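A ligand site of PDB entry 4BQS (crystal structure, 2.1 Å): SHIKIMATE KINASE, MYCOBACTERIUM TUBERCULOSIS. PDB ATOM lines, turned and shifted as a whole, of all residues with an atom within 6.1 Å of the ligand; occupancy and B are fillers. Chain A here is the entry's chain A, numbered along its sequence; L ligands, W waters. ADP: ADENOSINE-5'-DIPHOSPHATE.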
ATOM      1  N   GLY A   9      26.057   3.840 -14.746  1.00  0.00           N
ATOM      2  CA  GLY A   9      25.921   2.403 -15.060  1.00  0.00           C
ATOM      3  C   GLY A   9      26.632   2.047 -16.361  1.00  0.00           C
ATOM      4  O   GLY A   9      26.968   2.904 -17.182  1.00  0.00           O
ATOM      5  N   LEU A  10      26.878   0.764 -16.539  1.00  0.00           N
ATOM      6  CA  LEU A  10      27.445   0.268 -17.757  1.00  0.00           C
ATOM      7  C   LEU A  10      26.497   0.561 -18.913  1.00  0.00           C
ATOM      8  O   LEU A  10      25.312   0.854 -18.703  1.00  0.00           O
ATOM      9  CB  LEU A  10      27.650  -1.239 -17.659  1.00  0.00           C
ATOM     10  CG  LEU A  10      28.639  -1.718 -16.591  1.00  0.00           C
ATOM     11  CD1 LEU A  10      28.316  -3.161 -16.346  1.00  0.00           C
ATOM     12  CD2 LEU A  10      30.072  -1.534 -17.029  1.00  0.00           C
ATOM     13  N   PRO A  11      27.019   0.469 -20.143  1.00  0.00           N
ATOM     14  CA  PRO A  11      26.191   0.600 -21.312  1.00  0.00           C
ATOM     15  C   PRO A  11      25.205  -0.529 -21.271  1.00  0.00           C
ATOM     16  O   PRO A  11      25.529  -1.586 -20.772  1.00  0.00           O
ATOM     17  CB  PRO A  11      27.161   0.465 -22.473  1.00  0.00           C
ATOM     18  CG  PRO A  11      28.423  -0.078 -21.915  1.00  0.00           C
ATOM     19  CD  PRO A  11      28.447   0.227 -20.466  1.00  0.00           C
ATOM     20  N   GLY A  12      23.980  -0.282 -21.740  1.00  0.00           N
ATOM     21  CA  GLY A  12      22.938  -1.269 -21.631  1.00  0.00           C
ATOM     22  C   GLY A  12      22.136  -1.255 -20.319  1.00  0.00           C
ATOM     23  O   GLY A  12      21.070  -1.857 -20.280  1.00  0.00           O
ATOM     24  N   SER A  13      22.625  -0.567 -19.270  1.00  0.00           N
ATOM     25  CA  SER A  13      21.868  -0.422 -18.007  1.00  0.00           C
ATOM     26  C   SER A  13      20.587   0.416 -18.125  1.00  0.00           C
ATOM     27  O   SER A  13      19.764   0.372 -17.240  1.00  0.00           O
ATOM     28  CB  SER A  13      22.749   0.124 -16.864  1.00  0.00           C
ATOM     29  OG  SER A  13      23.286   1.429 -17.112  1.00  0.00           O
ATOM     30  N   GLY A  14      20.462   1.222 -19.174  1.00  0.00           N
ATOM     31  CA  GLY A  14      19.287   2.027 -19.448  1.00  0.00           C
ATOM     32  C   GLY A  14      19.413   3.520 -19.136  1.00  0.00           C
ATOM     33  O   GLY A  14      18.441   4.156 -18.819  1.00  0.00           O
ATOM     34  N   LYS A  15      20.600   4.082 -19.239  1.00  0.00           N
ATOM     35  CA  LYS A  15      20.802   5.462 -18.875  1.00  0.00           C
ATOM     36  C   LYS A  15      20.050   6.447 -19.762  1.00  0.00           C
ATOM     37  O   LYS A  15      19.582   7.448 -19.264  1.00  0.00           O
ATOM     38  CB  LYS A  15      22.273   5.836 -18.852  1.00  0.00           C
ATOM     39  CG  LYS A  15      23.090   4.993 -17.886  1.00  0.00           C
ATOM     40  CD  LYS A  15      24.482   5.542 -17.718  1.00  0.00           C
ATOM     41  CE  LYS A  15      25.313   5.364 -18.993  1.00  0.00           C
ATOM     42  NZ  LYS A  15      25.575   3.950 -19.348  1.00  0.00           N
ATOM     43  N   SER A  16      19.979   6.215 -21.062  1.00  0.00           N
ATOM     44  CA  SER A  16      19.153   7.076 -21.891  1.00  0.00           C
ATOM     45  C   SER A  16      17.661   6.726 -21.786  1.00  0.00           C
ATOM     46  O   SER A  16      16.867   7.607 -21.692  1.00  0.00           O
ATOM     47  CB  SER A  16      19.643   7.076 -23.335  1.00  0.00           C
ATOM     48  OG  SER A  16      19.889   5.779 -23.792  1.00  0.00           O
ATOM     49  N   THR A  17      17.290   5.455 -21.754  1.00  0.00           N
ATOM     50  CA  THR A  17      15.875   5.117 -21.578  1.00  0.00           C
ATOM     51  C   THR A  17      15.303   5.684 -20.251  1.00  0.00           C
ATOM     52  O   THR A  17      14.297   6.407 -20.217  1.00  0.00           O
ATOM     53  CB  THR A  17      15.659   3.601 -21.603  1.00  0.00           C
ATOM     54  OG1 THR A  17      16.281   3.033 -22.759  1.00  0.00           O
ATOM     55  CG2 THR A  17      14.170   3.258 -21.635  1.00  0.00           C
ATOM     56  N   ILE A  18      16.005   5.410 -19.149  1.00  0.00           N
ATOM     57  CA  ILE A  18      15.565   5.840 -17.852  1.00  0.00           C
ATOM     58  C   ILE A  18      15.779   7.321 -17.701  1.00  0.00           C
ATOM     59  O   ILE A  18      14.938   8.004 -17.114  1.00  0.00           O
ATOM     60  CB  ILE A  18      16.253   5.074 -16.693  1.00  0.00           C
ATOM     61  CG1 ILE A  18      16.075   3.574 -16.813  1.00  0.00           C
ATOM     62  CG2 ILE A  18      15.715   5.526 -15.344  1.00  0.00           C
ATOM     63  CD1 ILE A  18      14.654   3.124 -16.865  1.00  0.00           C
ATOM     64  N   LEU A 100      22.292   2.471 -12.003  1.00  0.00           N
ATOM     65  CA  LEU A 100      21.472   1.487 -12.729  1.00  0.00           C
ATOM     66  C   LEU A 100      22.198   0.167 -12.843  1.00  0.00           C
ATOM     67  O   LEU A 100      23.132   0.035 -13.621  1.00  0.00           O
ATOM     68  CB  LEU A 100      21.134   1.979 -14.127  1.00  0.00           C
ATOM     69  CG  LEU A 100      20.455   3.345 -14.176  1.00  0.00           C
ATOM     70  CD1 LEU A 100      20.085   3.731 -15.603  1.00  0.00           C
ATOM     71  CD2 LEU A 100      19.229   3.357 -13.289  1.00  0.00           C
ATOM     72  N   GLU A 106      22.042  -9.562 -19.484  1.00  0.00           N
ATOM     73  CA  GLU A 106      21.012  -8.662 -19.987  1.00  0.00           C
ATOM     74  C   GLU A 106      21.689  -7.432 -20.612  1.00  0.00           C
ATOM     75  O   GLU A 106      21.241  -6.954 -21.647  1.00  0.00           O
ATOM     76  CB  GLU A 106      20.015  -8.281 -18.881  1.00  0.00           C
ATOM     77  CG  GLU A 106      18.923  -7.306 -19.254  1.00  0.00           C
ATOM     78  CD  GLU A 106      18.054  -7.756 -20.428  1.00  0.00           C
ATOM     79  OE1 GLU A 106      18.215  -8.875 -20.943  1.00  0.00           O
ATOM     80  OE2 GLU A 106      17.206  -6.952 -20.859  1.00  0.00           O
ATOM     81  N   ARG A 109      22.868  -8.475 -23.975  1.00  0.00           N
ATOM     82  CA  ARG A 109      21.723  -8.632 -24.889  1.00  0.00           C
ATOM     83  C   ARG A 109      21.225  -7.290 -25.322  1.00  0.00           C
ATOM     84  O   ARG A 109      20.859  -7.109 -26.477  1.00  0.00           O
ATOM     85  CB  ARG A 109      20.554  -9.382 -24.229  1.00  0.00           C
ATOM     86  CG  ARG A 109      19.419  -9.663 -25.202  1.00  0.00           C
ATOM     87  CD  ARG A 109      18.097 -10.120 -24.584  1.00  0.00           C
ATOM     88  NE  ARG A 109      17.435  -9.130 -23.727  1.00  0.00           N
ATOM     89  CZ  ARG A 109      16.867  -7.997 -24.131  1.00  0.00           C
ATOM     90  NH1 ARG A 109      16.888  -7.648 -25.398  1.00  0.00           N
ATOM     91  NH2 ARG A 109      16.290  -7.183 -23.253  1.00  0.00           N
ATOM     92  N   ARG A 110      21.216  -6.328 -24.428  1.00  0.00           N
ATOM     93  CA  ARG A 110      20.690  -5.025 -24.746  1.00  0.00           C
ATOM     94  C   ARG A 110      21.654  -4.209 -25.537  1.00  0.00           C
ATOM     95  O   ARG A 110      21.218  -3.229 -26.106  1.00  0.00           O
ATOM     96  CB  ARG A 110      20.350  -4.198 -23.504  1.00  0.00           C
ATOM     97  CG  ARG A 110      19.207  -4.697 -22.649  1.00  0.00           C
ATOM     98  CD  ARG A 110      19.033  -3.746 -21.478  1.00  0.00           C
ATOM     99  NE  ARG A 110      18.045  -4.239 -20.534  1.00  0.00           N
ATOM    100  CZ  ARG A 110      17.759  -3.642 -19.375  1.00  0.00           C
ATOM    101  NH1 ARG A 110      18.388  -2.519 -19.002  1.00  0.00           N
ATOM    102  NH2 ARG A 110      16.872  -4.208 -18.577  1.00  0.00           N
ATOM    103  N   THR A 111      22.955  -4.568 -25.520  1.00  0.00           N
ATOM    104  CA  THR A 111      23.997  -3.839 -26.273  1.00  0.00           C
ATOM    105  C   THR A 111      24.462  -4.561 -27.561  1.00  0.00           C
ATOM    106  O   THR A 111      25.509  -4.250 -28.100  1.00  0.00           O
ATOM    107  CB  THR A 111      25.283  -3.579 -25.386  1.00  0.00           C
ATOM    108  OG1 THR A 111      25.737  -4.804 -24.828  1.00  0.00           O
ATOM    109  CG2 THR A 111      25.002  -2.617 -24.226  1.00  0.00           C
ATOM    110  N   ARG A 117      31.360   0.685 -30.053  1.00  0.00           N
ATOM    111  CA  ARG A 117      31.801   0.847 -28.676  1.00  0.00           C
ATOM    112  C   ARG A 117      33.252   0.402 -28.592  1.00  0.00           C
ATOM    113  O   ARG A 117      33.548  -0.791 -28.705  1.00  0.00           O
ATOM    114  CB  ARG A 117      30.923   0.050 -27.715  1.00  0.00           C
ATOM    115  CG  ARG A 117      29.426   0.347 -27.847  1.00  0.00           C
ATOM    116  CD  ARG A 117      28.686  -0.185 -26.612  1.00  0.00           C
ATOM    117  NE  ARG A 117      27.312   0.240 -26.598  1.00  0.00           N
ATOM    118  CZ  ARG A 117      26.305  -0.405 -27.159  1.00  0.00           C
ATOM    119  NH1 ARG A 117      26.490  -1.562 -27.784  1.00  0.00           N
ATOM    120  NH2 ARG A 117      25.100   0.134 -27.128  1.00  0.00           N
ATOM    121  N   THR A 150      17.741  -2.787 -12.913  1.00  0.00           N
ATOM    122  CA  THR A 150      16.996  -2.482 -14.109  1.00  0.00           C
ATOM    123  C   THR A 150      16.724  -3.757 -14.895  1.00  0.00           C
ATOM    124  O   THR A 150      16.133  -3.709 -15.961  1.00  0.00           O
ATOM    125  CB  THR A 150      17.659  -1.396 -15.001  1.00  0.00           C
ATOM    126  OG1 THR A 150      18.756  -1.963 -15.704  1.00  0.00           O
ATOM    127  CG2 THR A 150      18.101  -0.183 -14.206  1.00  0.00           C
ATOM    128  N   ASN A 151      17.079  -4.902 -14.302  1.00  0.00           N
ATOM    129  CA  ASN A 151      17.073  -6.176 -15.017  1.00  0.00           C
ATOM    130  C   ASN A 151      15.717  -6.492 -15.595  1.00  0.00           C
ATOM    131  O   ASN A 151      15.540  -6.452 -16.801  1.00  0.00           O
ATOM    132  CB  ASN A 151      17.522  -7.322 -14.102  1.00  0.00           C
ATOM    133  CG  ASN A 151      19.013  -7.571 -14.136  1.00  0.00           C
ATOM    134  OD1 ASN A 151      19.538  -8.053 -15.141  1.00  0.00           O
ATOM    135  ND2 ASN A 151      19.706  -7.313 -13.019  1.00  0.00           N
ATOM    136  N   ARG A 152      14.760  -6.818 -14.738  1.00  0.00           N
ATOM    137  CA  ARG A 152      13.464  -7.193 -15.250  1.00  0.00           C
ATOM    138  C   ARG A 152      12.733  -5.924 -15.587  1.00  0.00           C
ATOM    139  O   ARG A 152      12.188  -5.776 -16.675  1.00  0.00           O
ATOM    140  CB  ARG A 152      12.666  -8.088 -14.271  1.00  0.00           C
ATOM    141  CG  ARG A 152      12.196  -7.451 -12.973  1.00  0.00           C
ATOM    142  CD  ARG A 152      11.045  -8.257 -12.351  1.00  0.00           C
ATOM    143  NE  ARG A 152       9.692  -7.993 -12.907  1.00  0.00           N
ATOM    144  CZ  ARG A 152       8.907  -8.871 -13.558  1.00  0.00           C
ATOM    145  NH1 ARG A 152       9.278 -10.144 -13.792  1.00  0.00           N
ATOM    146  NH2 ARG A 152       7.703  -8.488 -13.986  1.00  0.00           N
ATOM    147  N   ARG A 153      12.786  -4.985 -14.646  1.00  0.00           N
ATOM    148  CA  ARG A 153      11.837  -3.886 -14.626  1.00  0.00           C
ATOM    149  C   ARG A 153      11.704  -3.219 -15.995  1.00  0.00           C
ATOM    150  O   ARG A 153      12.660  -2.604 -16.487  1.00  0.00           O
ATOM    151  CB  ARG A 153      12.232  -2.824 -13.589  1.00  0.00           C
ATOM    152  CG  ARG A 153      11.750  -3.031 -12.148  1.00  0.00           C
ATOM    153  CD  ARG A 153      11.423  -1.655 -11.555  1.00  0.00           C
ATOM    154  NE  ARG A 153      11.662  -1.472 -10.118  1.00  0.00           N
ATOM    155  CZ  ARG A 153      12.864  -1.494  -9.530  1.00  0.00           C
ATOM    156  NH1 ARG A 153      13.964  -1.714 -10.222  1.00  0.00           N
ATOM    157  NH2 ARG A 153      12.952  -1.301  -8.217  1.00  0.00           N
ATOM    158  N   ASN A 154      10.515  -3.365 -16.598  1.00  0.00           N
ATOM    159  CA  ASN A 154      10.054  -2.446 -17.641  1.00  0.00           C
ATOM    160  C   ASN A 154      10.310  -1.003 -17.176  1.00  0.00           C
ATOM    161  O   ASN A 154      10.122  -0.705 -15.972  1.00  0.00           O
ATOM    162  CB  ASN A 154       8.565  -2.643 -17.927  1.00  0.00           C
ATOM    163  CG  ASN A 154       7.748  -1.365 -17.731  1.00  0.00           C
ATOM    164  OD1 ASN A 154       7.757  -0.466 -18.572  1.00  0.00           O
ATOM    165  ND2 ASN A 154       7.063  -1.288 -16.607  1.00  0.00           N
ATOM    166  N   PRO A 155      10.766  -0.109 -18.087  1.00  0.00           N
ATOM    167  CA  PRO A 155      11.370   1.154 -17.646  1.00  0.00           C
ATOM    168  C   PRO A 155      10.520   2.021 -16.721  1.00  0.00           C
ATOM    169  O   PRO A 155      11.063   2.579 -15.758  1.00  0.00           O
ATOM    170  CB  PRO A 155      11.634   1.900 -18.955  1.00  0.00           C
ATOM    171  CG  PRO A 155      11.824   0.837 -19.954  1.00  0.00           C
ATOM    172  CD  PRO A 155      10.952  -0.323 -19.537  1.00  0.00           C
ATOM    173  N   VAL A 158      10.929   1.127 -13.238  1.00  0.00           N
ATOM    174  CA  VAL A 158      12.264   1.623 -12.793  1.00  0.00           C
ATOM    175  C   VAL A 158      12.147   3.075 -12.372  1.00  0.00           C
ATOM    176  O   VAL A 158      12.547   3.423 -11.267  1.00  0.00           O
ATOM    177  CB  VAL A 158      13.348   1.499 -13.900  1.00  0.00           C
ATOM    178  CG1 VAL A 158      14.649   2.241 -13.531  1.00  0.00           C
ATOM    179  CG2 VAL A 158      13.626   0.039 -14.130  1.00  0.00           C
HETATM  180  PB  ADP L   1      22.659   2.985 -21.854  1.00  0.00           P
HETATM  181  O1B ADP L   1      23.015   2.809 -20.375  1.00  0.00           O
HETATM  182  O2B ADP L   1      22.167   4.336 -22.270  1.00  0.00           O
HETATM  183  O3B ADP L   1      23.710   2.387 -22.726  1.00  0.00           O
HETATM  184  PA  ADP L   1      20.196   2.623 -23.156  1.00  0.00           P
HETATM  185  O1A ADP L   1      20.933   3.449 -24.183  1.00  0.00           O
HETATM  186  O2A ADP L   1      19.116   3.278 -22.350  1.00  0.00           O
HETATM  187  O3A ADP L   1      21.361   2.064 -22.154  1.00  0.00           O
HETATM  188  O5' ADP L   1      19.419   1.321 -23.686  1.00  0.00           O
HETATM  189  C5' ADP L   1      20.035   0.141 -24.163  1.00  0.00           C
HETATM  190  C4' ADP L   1      18.932  -0.760 -24.721  1.00  0.00           C
HETATM  191  O4' ADP L   1      18.235  -1.428 -23.672  1.00  0.00           O
HETATM  192  C3' ADP L   1      17.876   0.004 -25.502  1.00  0.00           C
HETATM  193  O3' ADP L   1      17.552  -0.786 -26.637  1.00  0.00           O
HETATM  194  C2' ADP L   1      16.693   0.106 -24.571  1.00  0.00           C
HETATM  195  O2' ADP L   1      15.427  -0.062 -25.203  1.00  0.00           O
HETATM  196  C1' ADP L   1      16.861  -1.081 -23.677  1.00  0.00           C
HETATM  197  N9  ADP L   1      16.438  -0.778 -22.297  1.00  0.00           N
HETATM  198  C8  ADP L   1      16.835   0.227 -21.471  1.00  0.00           C
HETATM  199  N7  ADP L   1      16.219   0.117 -20.265  1.00  0.00           N
HETATM  200  C5  ADP L   1      15.431  -0.972 -20.339  1.00  0.00           C
HETATM  201  C6  ADP L   1      14.507  -1.681 -19.452  1.00  0.00           C
HETATM  202  N6  ADP L   1      14.287  -1.224 -18.186  1.00  0.00           N
HETATM  203  N1  ADP L   1      13.908  -2.802 -19.944  1.00  0.00           N
HETATM  204  C2  ADP L   1      14.108  -3.273 -21.195  1.00  0.00           C
HETATM  205  N3  ADP L   1      14.921  -2.677 -22.050  1.00  0.00           N
HETATM  206  C4  ADP L   1      15.581  -1.556 -21.677  1.00  0.00           C
HETATM  207  O   HOH W   1      22.562   5.118 -25.075  1.00  0.00           O
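The backbone NH of Gly 12 lies within hydrogen-bond range of an oxygen (O3B) of the ligand (2.9 Å).
The side-chain hydroxyl (OG1) of Thr 17 lies within hydrogen-bond range of an oxygen (O2A) of the ligand (2.9 Å).
An oxygen (O1A) of the ligand is in hydrogen-bond range of the side-chain hydroxyl of Ser 16 (2.6 Å).
An oxygen (O1B) of the ligand lies within hydrogen-bond range of the backbone NH (N) of Lys 15 (3.0 Å).
An oxygen (O2A) of the ligand sits at hydrogen-bond distance from the backbone NH of Thr 17 (2.9 Å).
N6 of the ligand lies within hydrogen-bond range of O of Arg 153.
The backbone NH (N) of Ser 16 is in hydrogen-bond range of an oxygen (O2B) of the ligand (3.1 Å).
The backbone NH (N) of Gly 14 is in hydrogen-bond range of an oxygen (O3A) of the ligand, at 3.2 Å.
The side-chain amino group (NZ) of Lys 15 lies within salt-bridge range of an oxygen (O1B) of the ligand.
O of Leu 10 sits close to O1B of the ligand (3.4 Å).
Merely in contact with the ligand: Arg 110 (3.3 Å), Pro 11 (3.4 Å), Ser 13 (3.6 Å), Pro 155 (3.7 Å) and Thr 150 (3.8 Å).
Hydrophobic or aromatic side chains within 4 Å of the ligand: Pro 11 and Pro 155.
O of Leu 10 is in hydrogen-bond range of NZ of Lys 15.
O of Gly 9 sits at hydrogen-bond distance from NZ of Lys 15, at 2.8 Å.
NE of Arg 110 is in salt-bridge range of OE2 of Glu 106 (2.9 Å).
OG1 of Thr 150 lies within hydrogen-bond range of O of Ser 13 (3.0 Å).
NH1 of Arg 110 sits close to O of Gly 12 (3.0 Å).
The backbone carbonyl oxygen (O) of Thr 150 sits at hydrogen-bond distance from the guanidinium group (NH2) of Arg 110, at 2.8 Å.
The backbone carbonyl oxygen (O) of Leu 10 lies within hydrogen-bond range of the side-chain hydroxyl (OG) of Ser 13 (2.6 Å).
NH2 of Arg 110 sits at hydrogen-bond distance from O of Asn 151, 3.2 Å away.
Water W1 bridges an oxygen (O1A) of the ligand (2.5 Å) and the side-chain hydroxyl of Ser 16 (3.0 Å).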
